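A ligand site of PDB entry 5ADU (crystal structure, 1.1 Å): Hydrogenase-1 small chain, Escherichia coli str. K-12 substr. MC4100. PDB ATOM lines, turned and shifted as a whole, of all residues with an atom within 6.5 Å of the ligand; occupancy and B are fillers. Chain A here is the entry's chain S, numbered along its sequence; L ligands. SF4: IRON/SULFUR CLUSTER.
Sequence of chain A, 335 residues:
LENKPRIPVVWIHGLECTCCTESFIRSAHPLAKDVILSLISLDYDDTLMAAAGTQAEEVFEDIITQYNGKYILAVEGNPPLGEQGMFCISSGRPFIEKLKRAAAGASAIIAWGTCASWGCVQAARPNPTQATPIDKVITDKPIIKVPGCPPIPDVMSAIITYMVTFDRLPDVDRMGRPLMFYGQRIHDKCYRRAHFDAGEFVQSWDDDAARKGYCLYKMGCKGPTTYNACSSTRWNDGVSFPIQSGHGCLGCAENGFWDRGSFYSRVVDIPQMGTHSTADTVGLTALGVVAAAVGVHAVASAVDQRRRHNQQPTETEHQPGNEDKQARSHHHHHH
S3 of the ligand lies close to N of Leu 216 (3.5 Å).
A ring nitrogen (ND1) of His 187 is bound to an iron atom (FE3) of the ligand.
S2 of the ligand lies close to N of Arg 193.
The side-chain sulfur of Cys 221 is bound to an iron atom (FE2) of the ligand (2.3 Å).
An iron atom (FE4) of the ligand is bound by the side-chain sulfur (SG) of Cys 190 (2.3 Å).
SG of Cys 215 binds FE1 of the ligand, at 2.3 Å.
Arg 192 touches the ligand (C to S2, 3.8 Å).
Phe 196 touches the ligand (CB to S2, 3.9 Å).
Tyr 217 touches the ligand (CB to S4, 3.8 Å).
Gly 223 touches the ligand (CA to S1, 3.9 Å).
CD of Pro 224 touches S4 of the ligand, at 3.99 Å.
Ile 243 touches the ligand.
The side-chain hydroxyl (OH) of Tyr 191 sits at hydrogen-bond distance from the guanidinium group (NH2) of Arg 192, 3.1 Å away.
The side-chain sulfur (SG) of Cys 221 lies close to the backbone NH (N) of Cys 249.
The backbone NH of His 187 lies within hydrogen-bond range of the backbone carbonyl oxygen of Gly 223, 3.3 Å away.
The side-chain sulfur of Cys 215 sits close to the backbone NH of Tyr 217 (3.4 Å).
The side-chain carboxylate (OD1) of Asp 188 lies within salt-bridge range of the guanidinium group (NH1) of Arg 193 (3.2 Å).
The guanidinium group (NH1) of Arg 192 lies within hydrogen-bond range of the backbone carbonyl oxygen (O) of Tyr 214 (2.9 Å).
O of Ile 243 lies within hydrogen-bond range of NH2 of Arg 192, at 3.1 Å.
The side-chain sulfur of Cys 190 sits close to the backbone NH of Arg 192, at 3.5 Å.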
ATOM      1  N   ILE A 186      -8.094 -16.026   8.811  1.00  0.00           N
ATOM      2  CA  ILE A 186      -9.131 -15.113   8.323  1.00  0.00           C
ATOM      3  C   ILE A 186      -8.514 -13.745   7.984  1.00  0.00           C
ATOM      4  O   ILE A 186      -8.777 -13.146   6.909  1.00  0.00           O
ATOM      5  CB  ILE A 186     -10.266 -14.950   9.400  1.00  0.00           C
ATOM      6  CG1 ILE A 186     -11.073 -16.239   9.610  1.00  0.00           C
ATOM      7  CG2 ILE A 186     -11.178 -13.750   9.127  1.00  0.00           C
ATOM      8  CD1 ILE A 186     -11.858 -16.693   8.411  1.00  0.00           C
ATOM      9  N   HIS A 187      -7.675 -13.230   8.909  1.00  0.00           N
ATOM     10  CA  HIS A 187      -7.026 -11.882   8.792  1.00  0.00           C
ATOM     11  C   HIS A 187      -5.986 -11.816   7.653  1.00  0.00           C
ATOM     12  O   HIS A 187      -5.645 -10.688   7.244  1.00  0.00           O
ATOM     13  CB  HIS A 187      -6.386 -11.611  10.190  1.00  0.00           C
ATOM     14  CG  HIS A 187      -5.615 -10.328  10.407  1.00  0.00           C
ATOM     15  ND1 HIS A 187      -6.206  -9.076  10.599  1.00  0.00           N
ATOM     16  CD2 HIS A 187      -4.309 -10.157  10.674  1.00  0.00           C
ATOM     17  CE1 HIS A 187      -5.260  -8.194  10.919  1.00  0.00           C
ATOM     18  NE2 HIS A 187      -4.097  -8.828  10.956  1.00  0.00           N
ATOM     19  N   ASP A 188      -5.497 -12.963   7.150  1.00  0.00           N
ATOM     20  CA  ASP A 188      -4.558 -12.969   6.022  1.00  0.00           C
ATOM     21  C   ASP A 188      -5.231 -12.904   4.635  1.00  0.00           C
ATOM     22  O   ASP A 188      -4.521 -12.770   3.632  1.00  0.00           O
ATOM     23  CB  ASP A 188      -3.539 -14.047   6.218  1.00  0.00           C
ATOM     24  CG  ASP A 188      -2.581 -13.691   7.467  1.00  0.00           C
ATOM     25  OD1 ASP A 188      -2.382 -12.465   7.856  1.00  0.00           O
ATOM     26  OD2 ASP A 188      -1.991 -14.564   8.008  1.00  0.00           O
ATOM     27  N   CYS A 190      -8.494 -11.005   4.595  1.00  0.00           N
ATOM     28  CA  CYS A 190      -9.643 -10.121   4.909  1.00  0.00           C
ATOM     29  C   CYS A 190      -9.668  -8.847   4.082  1.00  0.00           C
ATOM     30  O   CYS A 190      -8.672  -8.099   4.027  1.00  0.00           O
ATOM     31  CB  CYS A 190      -9.650  -9.755   6.397  1.00  0.00           C
ATOM     32  SG  CYS A 190     -11.120  -8.767   6.900  1.00  0.00           S
ATOM     33  N   TYR A 191     -10.805  -8.561   3.444  1.00  0.00           N
ATOM     34  CA  TYR A 191     -10.960  -7.339   2.620  1.00  0.00           C
ATOM     35  C   TYR A 191     -10.923  -6.034   3.401  1.00  0.00           C
ATOM     36  O   TYR A 191     -10.801  -4.968   2.770  1.00  0.00           O
ATOM     37  CB  TYR A 191     -12.234  -7.445   1.706  1.00  0.00           C
ATOM     38  CG  TYR A 191     -13.537  -7.018   2.384  1.00  0.00           C
ATOM     39  CD1 TYR A 191     -14.018  -7.597   3.572  1.00  0.00           C
ATOM     40  CD2 TYR A 191     -14.348  -6.041   1.763  1.00  0.00           C
ATOM     41  CE1 TYR A 191     -15.202  -7.146   4.163  1.00  0.00           C
ATOM     42  CE2 TYR A 191     -15.527  -5.615   2.367  1.00  0.00           C
ATOM     43  CZ  TYR A 191     -15.946  -6.144   3.580  1.00  0.00           C
ATOM     44  OH  TYR A 191     -17.095  -5.691   4.225  1.00  0.00           O
ATOM     45  N   ARG A 192     -10.964  -6.066   4.734  1.00  0.00           N
ATOM     46  CA  ARG A 192     -10.792  -4.845   5.529  1.00  0.00           C
ATOM     47  C   ARG A 192      -9.343  -4.633   6.026  1.00  0.00           C
ATOM     48  O   ARG A 192      -9.061  -3.679   6.803  1.00  0.00           O
ATOM     49  CB  ARG A 192     -11.780  -4.800   6.709  1.00  0.00           C
ATOM     50  CG  ARG A 192     -13.243  -4.832   6.257  1.00  0.00           C
ATOM     51  CD  ARG A 192     -14.228  -4.614   7.392  1.00  0.00           C
ATOM     52  NE  ARG A 192     -15.619  -4.699   6.933  1.00  0.00           N
ATOM     53  CZ  ARG A 192     -16.697  -4.183   7.510  1.00  0.00           C
ATOM     54  NH1 ARG A 192     -16.609  -3.480   8.646  1.00  0.00           N
ATOM     55  NH2 ARG A 192     -17.891  -4.386   6.951  1.00  0.00           N
ATOM     56  N   ARG A 193      -8.395  -5.458   5.548  1.00  0.00           N
ATOM     57  CA  ARG A 193      -6.996  -5.350   6.020  1.00  0.00           C
ATOM     58  C   ARG A 193      -6.348  -4.000   5.680  1.00  0.00           C
ATOM     59  O   ARG A 193      -5.537  -3.520   6.482  1.00  0.00           O
ATOM     60  CB  ARG A 193      -6.174  -6.516   5.493  1.00  0.00           C
ATOM     61  CG  ARG A 193      -4.763  -6.642   6.008  1.00  0.00           C
ATOM     62  CD  ARG A 193      -4.707  -6.969   7.496  1.00  0.00           C
ATOM     63  NE  ARG A 193      -3.285  -7.004   7.752  1.00  0.00           N
ATOM     64  CZ  ARG A 193      -2.497  -8.062   7.782  1.00  0.00           C
ATOM     65  NH1 ARG A 193      -2.945  -9.312   7.764  1.00  0.00           N
ATOM     66  NH2 ARG A 193      -1.193  -7.844   7.868  1.00  0.00           N
ATOM     67  N   ALA A 194      -6.724  -3.366   4.562  1.00  0.00           N
ATOM     68  CA  ALA A 194      -6.222  -2.018   4.267  1.00  0.00           C
ATOM     69  C   ALA A 194      -6.483  -1.062   5.451  1.00  0.00           C
ATOM     70  O   ALA A 194      -5.626  -0.196   5.777  1.00  0.00           O
ATOM     71  CB  ALA A 194      -6.909  -1.458   3.024  1.00  0.00           C
ATOM     72  N   HIS A 195      -7.684  -1.170   6.042  1.00  0.00           N
ATOM     73  CA  HIS A 195      -8.049  -0.287   7.159  1.00  0.00           C
ATOM     74  C   HIS A 195      -7.251  -0.634   8.422  1.00  0.00           C
ATOM     75  O   HIS A 195      -6.749   0.290   9.122  1.00  0.00           O
ATOM     76  CB  HIS A 195      -9.562  -0.337   7.405  1.00  0.00           C
ATOM     77  CG  HIS A 195     -10.378   0.056   6.192  1.00  0.00           C
ATOM     78  ND1 HIS A 195     -10.209   1.271   5.549  1.00  0.00           N
ATOM     79  CD2 HIS A 195     -11.354  -0.593   5.511  1.00  0.00           C
ATOM     80  CE1 HIS A 195     -11.071   1.334   4.534  1.00  0.00           C
ATOM     81  NE2 HIS A 195     -11.774   0.210   4.494  1.00  0.00           N
ATOM     82  N   PHE A 196      -7.078  -1.920   8.739  1.00  0.00           N
ATOM     83  CA  PHE A 196      -6.185  -2.348   9.830  1.00  0.00           C
ATOM     84  C   PHE A 196      -4.785  -1.709   9.670  1.00  0.00           C
ATOM     85  O   PHE A 196      -4.245  -1.099  10.628  1.00  0.00           O
ATOM     86  CB  PHE A 196      -6.106  -3.877   9.892  1.00  0.00           C
ATOM     87  CG  PHE A 196      -5.212  -4.432  10.970  1.00  0.00           C
ATOM     88  CD1 PHE A 196      -3.874  -4.713  10.703  1.00  0.00           C
ATOM     89  CD2 PHE A 196      -5.699  -4.742  12.234  1.00  0.00           C
ATOM     90  CE1 PHE A 196      -3.035  -5.269  11.690  1.00  0.00           C
ATOM     91  CE2 PHE A 196      -4.875  -5.297  13.230  1.00  0.00           C
ATOM     92  CZ  PHE A 196      -3.542  -5.573  12.941  1.00  0.00           C
ATOM     93  N   PHE A 201     -10.300   2.291  12.269  1.00  0.00           N
ATOM     94  CA  PHE A 201     -11.060   1.327  13.097  1.00  0.00           C
ATOM     95  C   PHE A 201     -12.468   1.826  13.448  1.00  0.00           C
ATOM     96  O   PHE A 201     -12.651   3.005  13.798  1.00  0.00           O
ATOM     97  CB  PHE A 201     -10.335   1.055  14.401  1.00  0.00           C
ATOM     98  CG  PHE A 201      -8.953   0.453  14.244  1.00  0.00           C
ATOM     99  CD1 PHE A 201      -8.779  -0.822  13.736  1.00  0.00           C
ATOM    100  CD2 PHE A 201      -7.790   1.174  14.628  1.00  0.00           C
ATOM    101  CE1 PHE A 201      -7.509  -1.358  13.584  1.00  0.00           C
ATOM    102  CE2 PHE A 201      -6.541   0.606  14.502  1.00  0.00           C
ATOM    103  CZ  PHE A 201      -6.385  -0.660  13.972  1.00  0.00           C
ATOM    104  N   TYR A 214     -14.873   0.082   7.984  1.00  0.00           N
ATOM    105  CA  TYR A 214     -13.527   0.045   8.591  1.00  0.00           C
ATOM    106  C   TYR A 214     -13.307  -1.234   9.404  1.00  0.00           C
ATOM    107  O   TYR A 214     -14.248  -2.042   9.667  1.00  0.00           O
ATOM    108  CB  TYR A 214     -13.283   1.324   9.407  1.00  0.00           C
ATOM    109  CG  TYR A 214     -12.963   2.602   8.613  1.00  0.00           C
ATOM    110  CD1 TYR A 214     -13.031   2.676   7.220  1.00  0.00           C
ATOM    111  CD2 TYR A 214     -12.559   3.756   9.284  1.00  0.00           C
ATOM    112  CE1 TYR A 214     -12.691   3.855   6.509  1.00  0.00           C
ATOM    113  CE2 TYR A 214     -12.231   4.922   8.587  1.00  0.00           C
ATOM    114  CZ  TYR A 214     -12.350   4.962   7.211  1.00  0.00           C
ATOM    115  OH  TYR A 214     -11.998   6.168   6.583  1.00  0.00           O
ATOM    116  N   CYS A 215     -12.051  -1.478   9.796  1.00  0.00           N
ATOM    117  CA  CYS A 215     -11.640  -2.703  10.485  1.00  0.00           C
ATOM    118  C   CYS A 215     -12.304  -2.809  11.880  1.00  0.00           C
ATOM    119  O   CYS A 215     -12.525  -1.786  12.565  1.00  0.00           O
ATOM    120  CB  CYS A 215     -10.117  -2.757  10.574  1.00  0.00           C
ATOM    121  SG  CYS A 215      -9.386  -4.029  11.661  1.00  0.00           S
ATOM    122  N   LEU A 216     -12.585  -4.066  12.277  1.00  0.00           N
ATOM    123  CA  LEU A 216     -13.319  -4.421  13.511  1.00  0.00           C
ATOM    124  C   LEU A 216     -12.394  -4.876  14.664  1.00  0.00           C
ATOM    125  O   LEU A 216     -12.887  -5.343  15.709  1.00  0.00           O
ATOM    126  CB  LEU A 216     -14.384  -5.473  13.176  1.00  0.00           C
ATOM    127  CG  LEU A 216     -15.436  -4.964  12.188  1.00  0.00           C
ATOM    128  CD1 LEU A 216     -16.325  -6.101  11.686  1.00  0.00           C
ATOM    129  CD2 LEU A 216     -16.358  -3.904  12.756  1.00  0.00           C
ATOM    130  N   TYR A 217     -11.068  -4.695  14.537  1.00  0.00           N
ATOM    131  CA  TYR A 217     -10.099  -5.107  15.596  1.00  0.00           C
ATOM    132  C   TYR A 217     -10.422  -4.525  16.977  1.00  0.00           C
ATOM    133  O   TYR A 217     -10.357  -5.246  18.008  1.00  0.00           O
ATOM    134  CB  TYR A 217      -8.695  -4.673  15.164  1.00  0.00           C
ATOM    135  CG  TYR A 217      -7.625  -4.910  16.191  1.00  0.00           C
ATOM    136  CD1 TYR A 217      -7.167  -6.179  16.477  1.00  0.00           C
ATOM    137  CD2 TYR A 217      -7.076  -3.828  16.894  1.00  0.00           C
ATOM    138  CE1 TYR A 217      -6.147  -6.376  17.444  1.00  0.00           C
ATOM    139  CE2 TYR A 217      -6.095  -4.007  17.883  1.00  0.00           C
ATOM    140  CZ  TYR A 217      -5.661  -5.287  18.126  1.00  0.00           C
ATOM    141  OH  TYR A 217      -4.672  -5.470  19.069  1.00  0.00           O
ATOM    142  N   LYS A 218     -10.723  -3.220  17.033  1.00  0.00           N
ATOM    143  CA  LYS A 218     -11.027  -2.574  18.358  1.00  0.00           C
ATOM    144  C   LYS A 218     -12.387  -2.965  18.920  1.00  0.00           C
ATOM    145  O   LYS A 218     -12.651  -2.699  20.092  1.00  0.00           O
ATOM    146  CB  LYS A 218     -10.854  -1.032  18.290  1.00  0.00           C
ATOM    147  CG  LYS A 218      -9.421  -0.602  17.986  1.00  0.00           C
ATOM    148  CD  LYS A 218      -9.197   0.899  18.203  1.00  0.00           C
ATOM    149  CE  LYS A 218      -7.718   1.256  18.201  1.00  0.00           C
ATOM    150  NZ  LYS A 218      -7.497   2.741  18.242  1.00  0.00           N
ATOM    151  N   CYS A 221     -12.586  -8.248  17.100  1.00  0.00           N
ATOM    152  CA  CYS A 221     -12.414  -9.266  16.025  1.00  0.00           C
ATOM    153  C   CYS A 221     -11.254 -10.220  16.342  1.00  0.00           C
ATOM    154  O   CYS A 221     -10.106  -9.784  16.549  1.00  0.00           O
ATOM    155  CB  CYS A 221     -12.102  -8.552  14.682  1.00  0.00           C
ATOM    156  SG  CYS A 221     -12.057  -9.713  13.279  1.00  0.00           S
ATOM    157  N   LYS A 222     -11.535 -11.539  16.274  1.00  0.00           N
ATOM    158  CA  LYS A 222     -10.515 -12.585  16.518  1.00  0.00           C
ATOM    159  C   LYS A 222      -9.971 -13.185  15.212  1.00  0.00           C
ATOM    160  O   LYS A 222      -9.250 -14.228  15.222  1.00  0.00           O
ATOM    161  CB  LYS A 222     -11.081 -13.685  17.439  1.00  0.00           C
ATOM    162  CG  LYS A 222     -11.502 -13.145  18.846  1.00  0.00           C
ATOM    163  CD  LYS A 222     -10.428 -12.226  19.492  1.00  0.00           C
ATOM    164  CE  LYS A 222     -10.668 -11.705  20.875  1.00  0.00           C
ATOM    165  NZ  LYS A 222     -12.033 -11.183  21.156  1.00  0.00           N
ATOM    166  N   GLY A 223     -10.209 -12.505  14.078  1.00  0.00           N
ATOM    167  CA  GLY A 223      -9.628 -12.931  12.814  1.00  0.00           C
ATOM    168  C   GLY A 223      -8.105 -13.152  12.795  1.00  0.00           C
ATOM    169  O   GLY A 223      -7.638 -14.093  12.134  1.00  0.00           O
ATOM    170  N   PRO A 224      -7.333 -12.306  13.541  1.00  0.00           N
ATOM    171  CA  PRO A 224      -5.868 -12.496  13.545  1.00  0.00           C
ATOM    172  C   PRO A 224      -5.365 -13.843  14.109  1.00  0.00           C
ATOM    173  O   PRO A 224      -4.202 -14.172  13.837  1.00  0.00           O
ATOM    174  CB  PRO A 224      -5.382 -11.306  14.430  1.00  0.00           C
ATOM    175  CG  PRO A 224      -6.392 -10.240  14.141  1.00  0.00           C
ATOM    176  CD  PRO A 224      -7.691 -10.982  14.132  1.00  0.00           C
ATOM    177  N   PHE A 241     -20.015 -12.812   5.033  1.00  0.00           N
ATOM    178  CA  PHE A 241     -19.389 -13.523   6.160  1.00  0.00           C
ATOM    179  C   PHE A 241     -19.511 -12.594   7.374  1.00  0.00           C
ATOM    180  O   PHE A 241     -19.881 -11.416   7.223  1.00  0.00           O
ATOM    181  CB  PHE A 241     -17.937 -14.021   5.842  1.00  0.00           C
ATOM    182  CG  PHE A 241     -16.825 -12.981   5.823  1.00  0.00           C
ATOM    183  CD1 PHE A 241     -16.722 -12.035   4.830  1.00  0.00           C
ATOM    184  CD2 PHE A 241     -15.780 -13.093   6.755  1.00  0.00           C
ATOM    185  CE1 PHE A 241     -15.607 -11.162   4.780  1.00  0.00           C
ATOM    186  CE2 PHE A 241     -14.689 -12.202   6.719  1.00  0.00           C
ATOM    187  CZ  PHE A 241     -14.631 -11.254   5.717  1.00  0.00           C
ATOM    188  N   ILE A 243     -17.635 -10.589   9.286  1.00  0.00           N
ATOM    189  CA  ILE A 243     -16.996  -9.265   9.190  1.00  0.00           C
ATOM    190  C   ILE A 243     -17.655  -8.406   8.100  1.00  0.00           C
ATOM    191  O   ILE A 243     -17.849  -7.176   8.314  1.00  0.00           O
ATOM    192  CB  ILE A 243     -15.481  -9.460   8.967  1.00  0.00           C
ATOM    193  CG1 ILE A 243     -14.783  -9.959  10.263  1.00  0.00           C
ATOM    194  CG2 ILE A 243     -14.785  -8.176   8.439  1.00  0.00           C
ATOM    195  CD1 ILE A 243     -13.579 -10.887  10.030  1.00  0.00           C
ATOM    196  N   GLY A 248     -17.198  -8.470  14.337  1.00  0.00           N
ATOM    197  CA  GLY A 248     -15.913  -9.171  14.349  1.00  0.00           C
ATOM    198  C   GLY A 248     -16.077 -10.692  14.372  1.00  0.00           C
ATOM    199  O   GLY A 248     -17.053 -11.260  14.894  1.00  0.00           O
ATOM    200  N   CYS A 249     -15.060 -11.397  13.829  1.00  0.00           N
ATOM    201  CA  CYS A 249     -14.942 -12.855  14.033  1.00  0.00           C
ATOM    202  C   CYS A 249     -14.949 -13.160  15.563  1.00  0.00           C
ATOM    203  O   CYS A 249     -14.264 -12.485  16.358  1.00  0.00           O
ATOM    204  CB  CYS A 249     -13.627 -13.315  13.331  1.00  0.00           C
ATOM    205  SG  CYS A 249     -13.172 -15.082  13.491  1.00  0.00           S
HETATM  206 FE1  SF4 L   1      -9.689  -6.159  10.826  1.00  0.00          FE
HETATM  207 FE2  SF4 L   1     -10.755  -8.572  11.722  1.00  0.00          FE
HETATM  208 FE3  SF4 L   1      -8.231  -8.468  10.615  1.00  0.00          FE
HETATM  209 FE4  SF4 L   1     -10.413  -8.119   9.011  1.00  0.00          FE
HETATM  210  S1  SF4 L   1      -9.821 -10.064  10.198  1.00  0.00           S
HETATM  211  S2  SF4 L   1      -8.488  -6.826   8.962  1.00  0.00           S
HETATM  212  S3  SF4 L   1     -11.839  -6.936  10.409  1.00  0.00           S
HETATM  213  S4  SF4 L   1      -8.922  -7.506  12.603  1.00  0.00           S
